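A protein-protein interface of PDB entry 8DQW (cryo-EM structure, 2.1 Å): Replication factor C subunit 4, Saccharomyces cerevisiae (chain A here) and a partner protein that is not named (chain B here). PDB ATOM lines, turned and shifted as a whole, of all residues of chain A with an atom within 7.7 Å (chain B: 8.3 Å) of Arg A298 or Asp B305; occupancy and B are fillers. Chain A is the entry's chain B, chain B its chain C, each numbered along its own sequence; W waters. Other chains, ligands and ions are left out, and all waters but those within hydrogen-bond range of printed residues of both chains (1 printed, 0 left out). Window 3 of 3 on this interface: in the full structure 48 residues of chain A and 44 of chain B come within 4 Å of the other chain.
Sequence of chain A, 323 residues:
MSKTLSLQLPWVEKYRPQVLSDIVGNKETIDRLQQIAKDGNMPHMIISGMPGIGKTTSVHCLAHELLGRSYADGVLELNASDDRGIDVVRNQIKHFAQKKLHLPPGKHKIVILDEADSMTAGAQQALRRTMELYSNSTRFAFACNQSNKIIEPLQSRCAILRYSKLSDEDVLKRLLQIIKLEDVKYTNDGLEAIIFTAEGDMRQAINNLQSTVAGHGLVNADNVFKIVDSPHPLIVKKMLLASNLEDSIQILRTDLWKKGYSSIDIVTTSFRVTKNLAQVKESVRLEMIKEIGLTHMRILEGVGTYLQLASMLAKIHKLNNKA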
ATOM      1  N   GLU A 291      15.230  -4.942  11.935  1.00  0.00           N
ATOM      2  CA  GLU A 291      16.147  -5.616  12.851  1.00  0.00           C
ATOM      3  C   GLU A 291      17.574  -5.601  12.312  1.00  0.00           C
ATOM      4  O   GLU A 291      18.533  -5.385  13.067  1.00  0.00           O
ATOM      5  CB  GLU A 291      15.681  -7.051  13.104  1.00  0.00           C
ATOM      6  CG  GLU A 291      14.387  -7.159  13.906  1.00  0.00           C
ATOM      7  CD  GLU A 291      14.443  -6.424  15.235  1.00  0.00           C
ATOM      8  OE1 GLU A 291      15.557  -6.105  15.699  1.00  0.00           O
ATOM      9  OE2 GLU A 291      13.369  -6.163  15.817  1.00  0.00           O
ATOM     10  N   ILE A 292      17.733  -5.825  11.005  1.00  0.00           N
ATOM     11  CA  ILE A 292      19.057  -5.780  10.395  1.00  0.00           C
ATOM     12  C   ILE A 292      19.664  -4.393  10.552  1.00  0.00           C
ATOM     13  O   ILE A 292      20.855  -4.252  10.846  1.00  0.00           O
ATOM     14  CB  ILE A 292      18.975  -6.202   8.916  1.00  0.00           C
ATOM     15  CG1 ILE A 292      18.748  -7.712   8.809  1.00  0.00           C
ATOM     16  CG2 ILE A 292      20.241  -5.800   8.171  1.00  0.00           C
ATOM     17  CD1 ILE A 292      18.220  -8.158   7.461  1.00  0.00           C
ATOM     18  N   GLY A 293      18.859  -3.348  10.352  1.00  0.00           N
ATOM     19  CA  GLY A 293      19.365  -1.995  10.518  1.00  0.00           C
ATOM     20  C   GLY A 293      19.800  -1.705  11.941  1.00  0.00           C
ATOM     21  O   GLY A 293      20.828  -1.064  12.168  1.00  0.00           O
ATOM     22  N   LEU A 294      19.018  -2.162  12.923  1.00  0.00           N
ATOM     23  CA  LEU A 294      19.407  -1.950  14.315  1.00  0.00           C
ATOM     24  C   LEU A 294      20.714  -2.672  14.635  1.00  0.00           C
ATOM     25  O   LEU A 294      21.601  -2.113  15.297  1.00  0.00           O
ATOM     26  CB  LEU A 294      18.288  -2.413  15.250  1.00  0.00           C
ATOM     27  CG  LEU A 294      16.996  -1.592  15.182  1.00  0.00           C
ATOM     28  CD1 LEU A 294      15.836  -2.357  15.800  1.00  0.00           C
ATOM     29  CD2 LEU A 294      17.172  -0.238  15.860  1.00  0.00           C
ATOM     30  N   THR A 295      20.859  -3.912  14.160  1.00  0.00           N
ATOM     31  CA  THR A 295      22.103  -4.640  14.392  1.00  0.00           C
ATOM     32  C   THR A 295      23.276  -3.955  13.696  1.00  0.00           C
ATOM     33  O   THR A 295      24.391  -3.919  14.229  1.00  0.00           O
ATOM     34  CB  THR A 295      21.963  -6.088  13.917  1.00  0.00           C
ATOM     35  OG1 THR A 295      21.111  -6.807  14.817  1.00  0.00           O
ATOM     36  CG2 THR A 295      23.320  -6.772  13.872  1.00  0.00           C
ATOM     37  N   HIS A 296      23.043  -3.415  12.497  1.00  0.00           N
ATOM     38  CA  HIS A 296      24.085  -2.674  11.794  1.00  0.00           C
ATOM     39  C   HIS A 296      24.500  -1.437  12.579  1.00  0.00           C
ATOM     40  O   HIS A 296      25.690  -1.113  12.665  1.00  0.00           O
ATOM     41  CB  HIS A 296      23.584  -2.288  10.400  1.00  0.00           C
ATOM     42  CG  HIS A 296      24.615  -1.629   9.540  1.00  0.00           C
ATOM     43  ND1 HIS A 296      24.325  -1.127   8.289  1.00  0.00           N
ATOM     44  CD2 HIS A 296      25.931  -1.387   9.745  1.00  0.00           C
ATOM     45  CE1 HIS A 296      25.417  -0.604   7.762  1.00  0.00           C
ATOM     46  NE2 HIS A 296      26.406  -0.747   8.626  1.00  0.00           N
ATOM     47  N   MET A 297      23.528  -0.729  13.155  1.00  0.00           N
ATOM     48  CA  MET A 297      23.850   0.411  14.007  1.00  0.00           C
ATOM     49  C   MET A 297      24.719  -0.023  15.179  1.00  0.00           C
ATOM     50  O   MET A 297      25.704   0.644  15.514  1.00  0.00           O
ATOM     51  CB  MET A 297      22.567   1.065  14.518  1.00  0.00           C
ATOM     52  CG  MET A 297      22.797   2.340  15.314  1.00  0.00           C
ATOM     53  SD  MET A 297      21.263   3.176  15.761  1.00  0.00           S
ATOM     54  CE  MET A 297      20.493   1.938  16.802  1.00  0.00           C
ATOM     55  N   ARG A 298      24.370  -1.144  15.810  1.00  0.00           N
ATOM     56  CA  ARG A 298      25.167  -1.631  16.932  1.00  0.00           C
ATOM     57  C   ARG A 298      26.586  -1.980  16.491  1.00  0.00           C
ATOM     58  O   ARG A 298      27.556  -1.687  17.200  1.00  0.00           O
ATOM     59  CB  ARG A 298      24.485  -2.840  17.571  1.00  0.00           C
ATOM     60  CG  ARG A 298      23.322  -2.470  18.477  1.00  0.00           C
ATOM     61  CD  ARG A 298      23.054  -3.535  19.523  1.00  0.00           C
ATOM     62  NE  ARG A 298      21.765  -3.341  20.178  1.00  0.00           N
ATOM     63  CZ  ARG A 298      21.104  -4.282  20.837  1.00  0.00           C
ATOM     64  NH1 ARG A 298      21.584  -5.510  20.960  1.00  0.00           N
ATOM     65  NH2 ARG A 298      19.933  -3.983  21.393  1.00  0.00           N
ATOM     66  N   ILE A 299      26.726  -2.605  15.320  1.00  0.00           N
ATOM     67  CA  ILE A 299      28.049  -2.982  14.831  1.00  0.00           C
ATOM     68  C   ILE A 299      28.890  -1.744  14.541  1.00  0.00           C
ATOM     69  O   ILE A 299      30.078  -1.694  14.879  1.00  0.00           O
ATOM     70  CB  ILE A 299      27.923  -3.881  13.587  1.00  0.00           C
ATOM     71  CG1 ILE A 299      27.429  -5.272  13.987  1.00  0.00           C
ATOM     72  CG2 ILE A 299      29.261  -3.979  12.859  1.00  0.00           C
ATOM     73  CD1 ILE A 299      26.907  -6.084  12.829  1.00  0.00           C
ATOM     74  N   LEU A 300      28.296  -0.729  13.907  1.00  0.00           N
ATOM     75  CA  LEU A 300      29.056   0.472  13.573  1.00  0.00           C
ATOM     76  C   LEU A 300      29.593   1.161  14.821  1.00  0.00           C
ATOM     77  O   LEU A 300      30.653   1.794  14.771  1.00  0.00           O
ATOM     78  CB  LEU A 300      28.188   1.444  12.772  1.00  0.00           C
ATOM     79  CG  LEU A 300      27.910   1.072  11.313  1.00  0.00           C
ATOM     80  CD1 LEU A 300      27.024   2.122  10.656  1.00  0.00           C
ATOM     81  CD2 LEU A 300      29.202   0.896  10.528  1.00  0.00           C
ATOM     82  N   GLU A 301      28.879   1.056  15.943  1.00  0.00           N
ATOM     83  CA  GLU A 301      29.341   1.666  17.183  1.00  0.00           C
ATOM     84  C   GLU A 301      30.522   0.929  17.797  1.00  0.00           C
ATOM     85  O   GLU A 301      31.163   1.472  18.703  1.00  0.00           O
ATOM     86  CB  GLU A 301      28.193   1.731  18.190  1.00  0.00           C
ATOM     87  CG  GLU A 301      27.190   2.834  17.902  1.00  0.00           C
ATOM     88  CD  GLU A 301      25.813   2.526  18.452  1.00  0.00           C
ATOM     89  OE1 GLU A 301      25.058   1.783  17.791  1.00  0.00           O
ATOM     90  OE2 GLU A 301      25.485   3.027  19.547  1.00  0.00           O
ATOM     91  N   GLY A 302      30.823  -0.283  17.335  1.00  0.00           N
ATOM     92  CA  GLY A 302      31.980  -1.012  17.814  1.00  0.00           C
ATOM     93  C   GLY A 302      31.673  -2.399  18.339  1.00  0.00           C
ATOM     94  O   GLY A 302      32.588  -3.209  18.504  1.00  0.00           O
ATOM     95  N   VAL A 303      30.404  -2.692  18.613  1.00  0.00           N
ATOM     96  CA  VAL A 303      30.020  -4.015  19.138  1.00  0.00           C
ATOM     97  C   VAL A 303      29.733  -4.886  17.919  1.00  0.00           C
ATOM     98  O   VAL A 303      28.590  -5.117  17.521  1.00  0.00           O
ATOM     99  CB  VAL A 303      28.831  -3.931  20.101  1.00  0.00           C
ATOM    100  CG1 VAL A 303      28.752  -5.184  20.960  1.00  0.00           C
ATOM    101  CG2 VAL A 303      28.933  -2.683  20.973  1.00  0.00           C
ATOM    102  N   GLY A 304      30.807  -5.391  17.315  1.00  0.00           N
ATOM    103  CA  GLY A 304      30.706  -6.303  16.191  1.00  0.00           C
ATOM    104  C   GLY A 304      30.878  -7.758  16.571  1.00  0.00           C
ATOM    105  O   GLY A 304      31.663  -8.472  15.940  1.00  0.00           O
ATOM    106  N   THR A 305      30.156  -8.219  17.584  1.00  0.00           N
ATOM    107  CA  THR A 305      30.381  -9.538  18.153  1.00  0.00           C
ATOM    108  C   THR A 305      29.428 -10.568  17.558  1.00  0.00           C
ATOM    109  O   THR A 305      28.368 -10.240  17.019  1.00  0.00           O
ATOM    110  CB  THR A 305      30.224  -9.507  19.676  1.00  0.00           C
ATOM    111  OG1 THR A 305      28.848  -9.296  20.015  1.00  0.00           O
ATOM    112  CG2 THR A 305      31.074  -8.395  20.283  1.00  0.00           C
ATOM    113  N   LEU A 307      27.646 -12.538  19.206  1.00  0.00           N
ATOM    114  CA  LEU A 307      26.407 -12.527  19.976  1.00  0.00           C
ATOM    115  C   LEU A 307      25.382 -11.585  19.355  1.00  0.00           C
ATOM    116  O   LEU A 307      24.182 -11.882  19.347  1.00  0.00           O
ATOM    117  CB  LEU A 307      26.704 -12.135  21.426  1.00  0.00           C
ATOM    118  CG  LEU A 307      25.514 -11.929  22.368  1.00  0.00           C
ATOM    119  CD1 LEU A 307      24.928 -13.266  22.792  1.00  0.00           C
ATOM    120  CD2 LEU A 307      25.943 -11.128  23.587  1.00  0.00           C
ATOM    121  N   GLN A 308      25.833 -10.440  18.837  1.00  0.00           N
ATOM    122  CA  GLN A 308      24.906  -9.505  18.203  1.00  0.00           C
ATOM    123  C   GLN A 308      24.244 -10.130  16.978  1.00  0.00           C
ATOM    124  O   GLN A 308      23.031  -9.994  16.779  1.00  0.00           O
ATOM    125  CB  GLN A 308      25.643  -8.221  17.818  1.00  0.00           C
ATOM    126  CG  GLN A 308      26.239  -7.453  18.997  1.00  0.00           C
ATOM    127  CD  GLN A 308      25.212  -7.099  20.059  1.00  0.00           C
ATOM    128  OE1 GLN A 308      24.127  -6.608  19.751  1.00  0.00           O
ATOM    129  NE2 GLN A 308      25.555  -7.346  21.318  1.00  0.00           N
ATOM    130  N   SER A 311      21.698 -12.680  18.097  1.00  0.00           N
ATOM    131  CA  SER A 311      20.476 -12.018  18.545  1.00  0.00           C
ATOM    132  C   SER A 311      19.655 -11.515  17.363  1.00  0.00           C
ATOM    133  O   SER A 311      18.420 -11.584  17.382  1.00  0.00           O
ATOM    134  CB  SER A 311      20.819 -10.864  19.487  1.00  0.00           C
ATOM    135  OG  SER A 311      19.709 -10.003  19.662  1.00  0.00           O
ATOM    136  N   MET A 312      20.322 -10.991  16.333  1.00  0.00           N
ATOM    137  CA  MET A 312      19.612 -10.587  15.124  1.00  0.00           C
ATOM    138  C   MET A 312      18.870 -11.770  14.511  1.00  0.00           C
ATOM    139  O   MET A 312      17.702 -11.650  14.117  1.00  0.00           O
ATOM    140  CB  MET A 312      20.599  -9.991  14.118  1.00  0.00           C
ATOM    141  CG  MET A 312      19.958  -9.415  12.863  1.00  0.00           C
ATOM    142  SD  MET A 312      21.144  -9.131  11.532  1.00  0.00           S
ATOM    143  CE  MET A 312      21.580 -10.812  11.084  1.00  0.00           C
ATOM    144  N   LYS A 315      15.802 -12.601  16.620  1.00  0.00           N
ATOM    145  CA  LYS A 315      14.702 -11.674  16.369  1.00  0.00           C
ATOM    146  C   LYS A 315      14.024 -11.971  15.036  1.00  0.00           C
ATOM    147  O   LYS A 315      12.789 -11.959  14.939  1.00  0.00           O
ATOM    148  CB  LYS A 315      15.212 -10.234  16.398  1.00  0.00           C
ATOM    149  CG  LYS A 315      15.038  -9.542  17.741  1.00  0.00           C
ATOM    150  CD  LYS A 315      15.847  -8.256  17.819  1.00  0.00           C
ATOM    151  CE  LYS A 315      16.437  -8.047  19.203  1.00  0.00           C
ATOM    152  NZ  LYS A 315      15.385  -8.029  20.256  1.00  0.00           N
ATOM    153  N   ILE B 278      30.141 -12.589  30.855  1.00  0.00           N
ATOM    154  CA  ILE B 278      29.017 -12.786  29.943  1.00  0.00           C
ATOM    155  C   ILE B 278      29.463 -13.561  28.711  1.00  0.00           C
ATOM    156  O   ILE B 278      28.762 -14.464  28.241  1.00  0.00           O
ATOM    157  CB  ILE B 278      28.394 -11.430  29.558  1.00  0.00           C
ATOM    158  CG1 ILE B 278      27.725 -10.784  30.772  1.00  0.00           C
ATOM    159  CG2 ILE B 278      27.388 -11.609  28.427  1.00  0.00           C
ATOM    160  CD1 ILE B 278      27.418  -9.308  30.587  1.00  0.00           C
ATOM    161  N   HIS B 298      15.141 -15.722  24.082  1.00  0.00           N
ATOM    162  CA  HIS B 298      15.241 -14.807  25.215  1.00  0.00           C
ATOM    163  C   HIS B 298      16.692 -14.602  25.629  1.00  0.00           C
ATOM    164  O   HIS B 298      17.140 -13.465  25.823  1.00  0.00           O
ATOM    165  CB  HIS B 298      14.418 -15.329  26.396  1.00  0.00           C
ATOM    166  CG  HIS B 298      12.949 -15.421  26.122  1.00  0.00           C
ATOM    167  ND1 HIS B 298      12.070 -16.042  26.983  1.00  0.00           N
ATOM    168  CD2 HIS B 298      12.199 -14.945  25.100  1.00  0.00           C
ATOM    169  CE1 HIS B 298      10.846 -15.960  26.495  1.00  0.00           C
ATOM    170  NE2 HIS B 298      10.897 -15.299  25.353  1.00  0.00           N
ATOM    171  N   LEU B 299      17.445 -15.696  25.765  1.00  0.00           N
ATOM    172  CA  LEU B 299      18.840 -15.584  26.174  1.00  0.00           C
ATOM    173  C   LEU B 299      19.608 -14.676  25.226  1.00  0.00           C
ATOM    174  O   LEU B 299      20.258 -13.715  25.655  1.00  0.00           O
ATOM    175  CB  LEU B 299      19.488 -16.969  26.222  1.00  0.00           C
ATOM    176  CG  LEU B 299      19.249 -17.803  27.481  1.00  0.00           C
ATOM    177  CD1 LEU B 299      19.553 -19.269  27.215  1.00  0.00           C
ATOM    178  CD2 LEU B 299      20.081 -17.281  28.641  1.00  0.00           C
ATOM    179  N   LEU B 300      19.527 -14.957  23.925  1.00  0.00           N
ATOM    180  CA  LEU B 300      20.311 -14.205  22.954  1.00  0.00           C
ATOM    181  C   LEU B 300      19.933 -12.731  22.973  1.00  0.00           C
ATOM    182  O   LEU B 300      20.805 -11.858  23.069  1.00  0.00           O
ATOM    183  CB  LEU B 300      20.113 -14.798  21.559  1.00  0.00           C
ATOM    184  CG  LEU B 300      20.894 -16.083  21.266  1.00  0.00           C
ATOM    185  CD1 LEU B 300      20.404 -16.724  19.975  1.00  0.00           C
ATOM    186  CD2 LEU B 300      22.390 -15.813  21.200  1.00  0.00           C
ATOM    187  N   THR B 301      18.633 -12.429  22.901  1.00  0.00           N
ATOM    188  CA  THR B 301      18.219 -11.031  22.820  1.00  0.00           C
ATOM    189  C   THR B 301      18.615 -10.267  24.080  1.00  0.00           C
ATOM    190  O   THR B 301      19.217  -9.187  24.002  1.00  0.00           O
ATOM    191  CB  THR B 301      16.709 -10.940  22.583  1.00  0.00           C
ATOM    192  OG1 THR B 301      16.016 -11.758  23.535  1.00  0.00           O
ATOM    193  CG2 THR B 301      16.362 -11.398  21.172  1.00  0.00           C
ATOM    194  N   LYS B 302      18.292 -10.816  25.255  1.00  0.00           N
ATOM    195  CA  LYS B 302      18.577 -10.102  26.495  1.00  0.00           C
ATOM    196  C   LYS B 302      20.077  -9.927  26.704  1.00  0.00           C
ATOM    197  O   LYS B 302      20.531  -8.849  27.112  1.00  0.00           O
ATOM    198  CB  LYS B 302      17.947 -10.838  27.677  1.00  0.00           C
ATOM    199  CG  LYS B 302      16.430 -10.719  27.736  1.00  0.00           C
ATOM    200  CD  LYS B 302      15.859 -11.466  28.935  1.00  0.00           C
ATOM    201  CE  LYS B 302      14.404 -11.099  29.204  1.00  0.00           C
ATOM    202  NZ  LYS B 302      14.195  -9.633  29.372  1.00  0.00           N
ATOM    203  N   LEU B 303      20.869 -10.969  26.434  1.00  0.00           N
ATOM    204  CA  LEU B 303      22.305 -10.860  26.653  1.00  0.00           C
ATOM    205  C   LEU B 303      22.946  -9.898  25.660  1.00  0.00           C
ATOM    206  O   LEU B 303      23.877  -9.168  26.016  1.00  0.00           O
ATOM    207  CB  LEU B 303      22.955 -12.243  26.572  1.00  0.00           C
ATOM    208  CG  LEU B 303      22.610 -13.203  27.716  1.00  0.00           C
ATOM    209  CD1 LEU B 303      23.323 -14.534  27.531  1.00  0.00           C
ATOM    210  CD2 LEU B 303      22.947 -12.601  29.078  1.00  0.00           C
ATOM    211  N   ALA B 304      22.462  -9.870  24.415  1.00  0.00           N
ATOM    212  CA  ALA B 304      22.966  -8.885  23.463  1.00  0.00           C
ATOM    213  C   ALA B 304      22.642  -7.469  23.921  1.00  0.00           C
ATOM    214  O   ALA B 304      23.480  -6.564  23.810  1.00  0.00           O
ATOM    215  CB  ALA B 304      22.383  -9.146  22.075  1.00  0.00           C
ATOM    216  N   ASP B 305      21.428  -7.258  24.438  1.00  0.00           N
ATOM    217  CA  ASP B 305      21.079  -5.940  24.961  1.00  0.00           C
ATOM    218  C   ASP B 305      21.989  -5.551  26.121  1.00  0.00           C
ATOM    219  O   ASP B 305      22.449  -4.405  26.205  1.00  0.00           O
ATOM    220  CB  ASP B 305      19.615  -5.921  25.404  1.00  0.00           C
ATOM    221  CG  ASP B 305      18.651  -5.844  24.236  1.00  0.00           C
ATOM    222  OD1 ASP B 305      19.099  -5.556  23.106  1.00  0.00           O
ATOM    223  OD2 ASP B 305      17.441  -6.069  24.449  1.00  0.00           O
ATOM    224  N   ILE B 306      22.256  -6.492  27.028  1.00  0.00           N
ATOM    225  CA  ILE B 306      23.126  -6.197  28.164  1.00  0.00           C
ATOM    226  C   ILE B 306      24.534  -5.863  27.687  1.00  0.00           C
ATOM    227  O   ILE B 306      25.175  -4.943  28.206  1.00  0.00           O
ATOM    228  CB  ILE B 306      23.131  -7.369  29.163  1.00  0.00           C
ATOM    229  CG1 ILE B 306      21.750  -7.528  29.805  1.00  0.00           C
ATOM    230  CG2 ILE B 306      24.190  -7.144  30.236  1.00  0.00           C
ATOM    231  CD1 ILE B 306      21.507  -8.897  30.400  1.00  0.00           C
ATOM    232  N   GLU B 307      25.046  -6.615  26.710  1.00  0.00           N
ATOM    233  CA  GLU B 307      26.374  -6.323  26.178  1.00  0.00           C
ATOM    234  C   GLU B 307      26.423  -4.928  25.565  1.00  0.00           C
ATOM    235  O   GLU B 307      27.374  -4.169  25.796  1.00  0.00           O
ATOM    236  CB  GLU B 307      26.771  -7.377  25.143  1.00  0.00           C
ATOM    237  CG  GLU B 307      28.016  -7.021  24.335  1.00  0.00           C
ATOM    238  CD  GLU B 307      28.493  -8.160  23.452  1.00  0.00           C
ATOM    239  OE1 GLU B 307      28.118  -8.191  22.262  1.00  0.00           O
ATOM    240  OE2 GLU B 307      29.250  -9.021  23.948  1.00  0.00           O
ATOM    241  N   TYR B 308      25.402  -4.570  24.783  1.00  0.00           N
ATOM    242  CA  TYR B 308      25.377  -3.239  24.185  1.00  0.00           C
ATOM    243  C   TYR B 308      25.342  -2.158  25.258  1.00  0.00           C
ATOM    244  O   TYR B 308      26.038  -1.141  25.148  1.00  0.00           O
ATOM    245  CB  TYR B 308      24.177  -3.102  23.248  1.00  0.00           C
ATOM    246  CG  TYR B 308      24.061  -1.732  22.619  1.00  0.00           C
ATOM    247  CD1 TYR B 308      25.078  -1.222  21.824  1.00  0.00           C
ATOM    248  CD2 TYR B 308      22.934  -0.948  22.824  1.00  0.00           C
ATOM    249  CE1 TYR B 308      24.974   0.031  21.249  1.00  0.00           C
ATOM    250  CE2 TYR B 308      22.821   0.303  22.252  1.00  0.00           C
ATOM    251  CZ  TYR B 308      23.842   0.789  21.467  1.00  0.00           C
ATOM    252  OH  TYR B 308      23.730   2.036  20.899  1.00  0.00           O
ATOM    253  N   SER B 309      24.535  -2.357  26.302  1.00  0.00           N
ATOM    254  CA  SER B 309      24.480  -1.376  27.384  1.00  0.00           C
ATOM    255  C   SER B 309      25.827  -1.252  28.086  1.00  0.00           C
ATOM    256  O   SER B 309      26.281  -0.142  28.385  1.00  0.00           O
ATOM    257  CB  SER B 309      23.388  -1.758  28.382  1.00  0.00           C
ATOM    258  OG  SER B 309      23.729  -1.339  29.692  1.00  0.00           O
ATOM    259  N   ILE B 310      26.485  -2.383  28.352  1.00  0.00           N
ATOM    260  CA  ILE B 310      27.795  -2.353  28.998  1.00  0.00           C
ATOM    261  C   ILE B 310      28.795  -1.604  28.129  1.00  0.00           C
ATOM    262  O   ILE B 310      29.694  -0.923  28.636  1.00  0.00           O
ATOM    263  CB  ILE B 310      28.278  -3.784  29.303  1.00  0.00           C
ATOM    264  CG1 ILE B 310      27.494  -4.377  30.477  1.00  0.00           C
ATOM    265  CG2 ILE B 310      29.774  -3.792  29.605  1.00  0.00           C
ATOM    266  CD1 ILE B 310      27.589  -5.887  30.571  1.00  0.00           C
ATOM    267  N   SER B 311      28.659  -1.722  26.806  1.00  0.00           N
ATOM    268  CA  SER B 311      29.603  -1.059  25.912  1.00  0.00           C
ATOM    269  C   SER B 311      29.615   0.452  26.120  1.00  0.00           C
ATOM    270  O   SER B 311      30.601   1.115  25.773  1.00  0.00           O
ATOM    271  CB  SER B 311      29.269  -1.388  24.457  1.00  0.00           C
ATOM    272  OG  SER B 311      28.466  -0.379  23.872  1.00  0.00           O
ATOM    273  N   LYS B 312      28.542   1.016  26.674  1.00  0.00           N
ATOM    274  CA  LYS B 312      28.440   2.451  26.908  1.00  0.00           C
ATOM    275  C   LYS B 312      28.675   2.837  28.364  1.00  0.00           C
ATOM    276  O   LYS B 312      28.526   4.013  28.711  1.00  0.00           O
ATOM    277  CB  LYS B 312      27.070   2.961  26.458  1.00  0.00           C
ATOM    278  CG  LYS B 312      26.653   2.482  25.079  1.00  0.00           C
ATOM    279  CD  LYS B 312      25.760   3.498  24.381  1.00  0.00           C
ATOM    280  CE  LYS B 312      24.319   3.424  24.871  1.00  0.00           C
ATOM    281  NZ  LYS B 312      23.776   2.037  24.872  1.00  0.00           N
ATOM    282  N   GLN B 319      23.751  -4.081  35.939  1.00  0.00           N
ATOM    283  CA  GLN B 319      23.976  -4.935  34.777  1.00  0.00           C
ATOM    284  C   GLN B 319      24.165  -6.395  35.181  1.00  0.00           C
ATOM    285  O   GLN B 319      23.641  -7.301  34.519  1.00  0.00           O
ATOM    286  CB  GLN B 319      25.183  -4.422  33.989  1.00  0.00           C
ATOM    287  CG  GLN B 319      24.858  -3.226  33.102  1.00  0.00           C
ATOM    288  CD  GLN B 319      26.053  -2.324  32.858  1.00  0.00           C
ATOM    289  OE1 GLN B 319      27.169  -2.626  33.276  1.00  0.00           O
ATOM    290  NE2 GLN B 319      25.822  -1.210  32.171  1.00  0.00           N
ATOM    291  N   ALA B 322      20.898  -7.772  36.106  1.00  0.00           N
ATOM    292  CA  ALA B 322      20.138  -7.968  34.880  1.00  0.00           C
ATOM    293  C   ALA B 322      20.530  -9.268  34.197  1.00  0.00           C
ATOM    294  O   ALA B 322      19.671  -9.987  33.682  1.00  0.00           O
ATOM    295  CB  ALA B 322      20.351  -6.785  33.939  1.00  0.00           C
ATOM    296  N   VAL B 323      21.827  -9.577  34.166  1.00  0.00           N
ATOM    297  CA  VAL B 323      22.267 -10.844  33.584  1.00  0.00           C
ATOM    298  C   VAL B 323      21.636 -12.012  34.334  1.00  0.00           C
ATOM    299  O   VAL B 323      21.098 -12.953  33.729  1.00  0.00           O
ATOM    300  CB  VAL B 323      23.804 -10.935  33.593  1.00  0.00           C
ATOM    301  CG1 VAL B 323      24.262 -12.343  33.231  1.00  0.00           C
ATOM    302  CG2 VAL B 323      24.402  -9.919  32.636  1.00  0.00           C
HETATM  303  O   HOH W   1      19.288  -7.739  21.760  1.00  0.00           O
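The backbone carbonyl oxygen of Ala B304 is in hydrogen-bond range of the side-chain amide nitrogen of Gln A308, 3.3 Å away. The side-chain carboxylate (OE1) of Glu B307 sits at hydrogen-bond distance from the side-chain amide nitrogen (NE2) of Gln A308, 2.9 Å away. The side-chain hydroxyl (OH) of Tyr B308 lies within hydrogen-bond range of the side-chain carboxylate (OE2) of Glu A301 (2.4 Å). The guanidinium group (NH2) of Arg A298 lies within salt-bridge range of the side-chain carboxylate (OD1) of Asp B305, at 2.5 Å. OG1 of Thr A305 sits at hydrogen-bond distance from OE1 of Glu B307 (2.6 Å).
OG1 of Thr A305 lies close to N of Gln A308 (3.4 Å). OG of Ser B311 sits at hydrogen-bond distance from O of Tyr B308. The backbone carbonyl oxygen of Met A297 sits close to the side-chain carboxylate of Glu A301 (2.6 Å). The backbone carbonyl oxygen (O) of Arg A298 lies within hydrogen-bond range of the backbone NH (N) of Val A303, at 3.3 Å. The guanidinium group of Arg A298 sits at hydrogen-bond distance from the side-chain amide oxygen of Gln A308 (3.0 Å).
Of chain B, only Ala B304 (3.6 Å), Asp B305 (2.5 Å) and Tyr B308 (3.7 Å) come within 4 Å of Arg A298. Of the printed residues of chain B, Glu A301 touches Tyr B308 (2.4 Å). Of the printed residues of chain B, Thr A305 touches Glu B307. Of the printed residues of chain B, Leu A307 touches Leu B300 (3.9 Å), Leu B303 (3.7 Å), Ala B304 (3.7 Å) and Glu B307 (3.9 Å). Of chain A, only Arg A298 (3.6 Å), Leu A307 (3.7 Å), Gln A308 (3.3 Å) and Ser A311 (3.5 Å) come within 4 Å of Ala B304. Asp B305 touches one residue of chain A. Of the printed residues of chain A, Tyr B308 touches Arg A298 and Glu A301. Of the printed residues of chain A, Ser B311 touches Val A303 (3.7 Å). Lys B312 touches none of the printed residues of chain A. The nearest residue of chain A that does not touch Asp B305 is Lys A315 (5.1 Å).
Arg A298 touches Tyr B308. Val A303 touches Glu B307. CB of Ser B311 touches CG2 of Val A303, 3.7 Å away. Leu B300 touches Leu A307 (CD2 to CD1, 3.9 Å). Leu B303 touches Leu A307 (O to CD2, 3.7 Å). CA of Ala B304 touches CD2 of Leu A307, at 3.7 Å. Leu A307 touches Glu B307 (CD2 to OE1, 3.9 Å). Leu B300 touches Ser A311 (O to CB, 3.7 Å). OG of Ser A311 touches CA of Thr B301 (3.6 Å). CG2 of Thr B301 touches NZ of Lys A315, 3.6 Å away.
Water W1 lies within hydrogen-bond range of OD1 of Asp B305, O of Thr B301, OG of Ser A311 and NH1 of Arg A298.
Of the 20 printed residues of chain A, 8 touch a printed residue of chain B. Among the printed residues, 17 pairs touch across the chains. Among the printed residues, Asp or Glu carboxylates within 4 Å of a Lys or Arg side-chain nitrogen of the other chain: Arg A298 with Asp B305 (2.5 Å).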
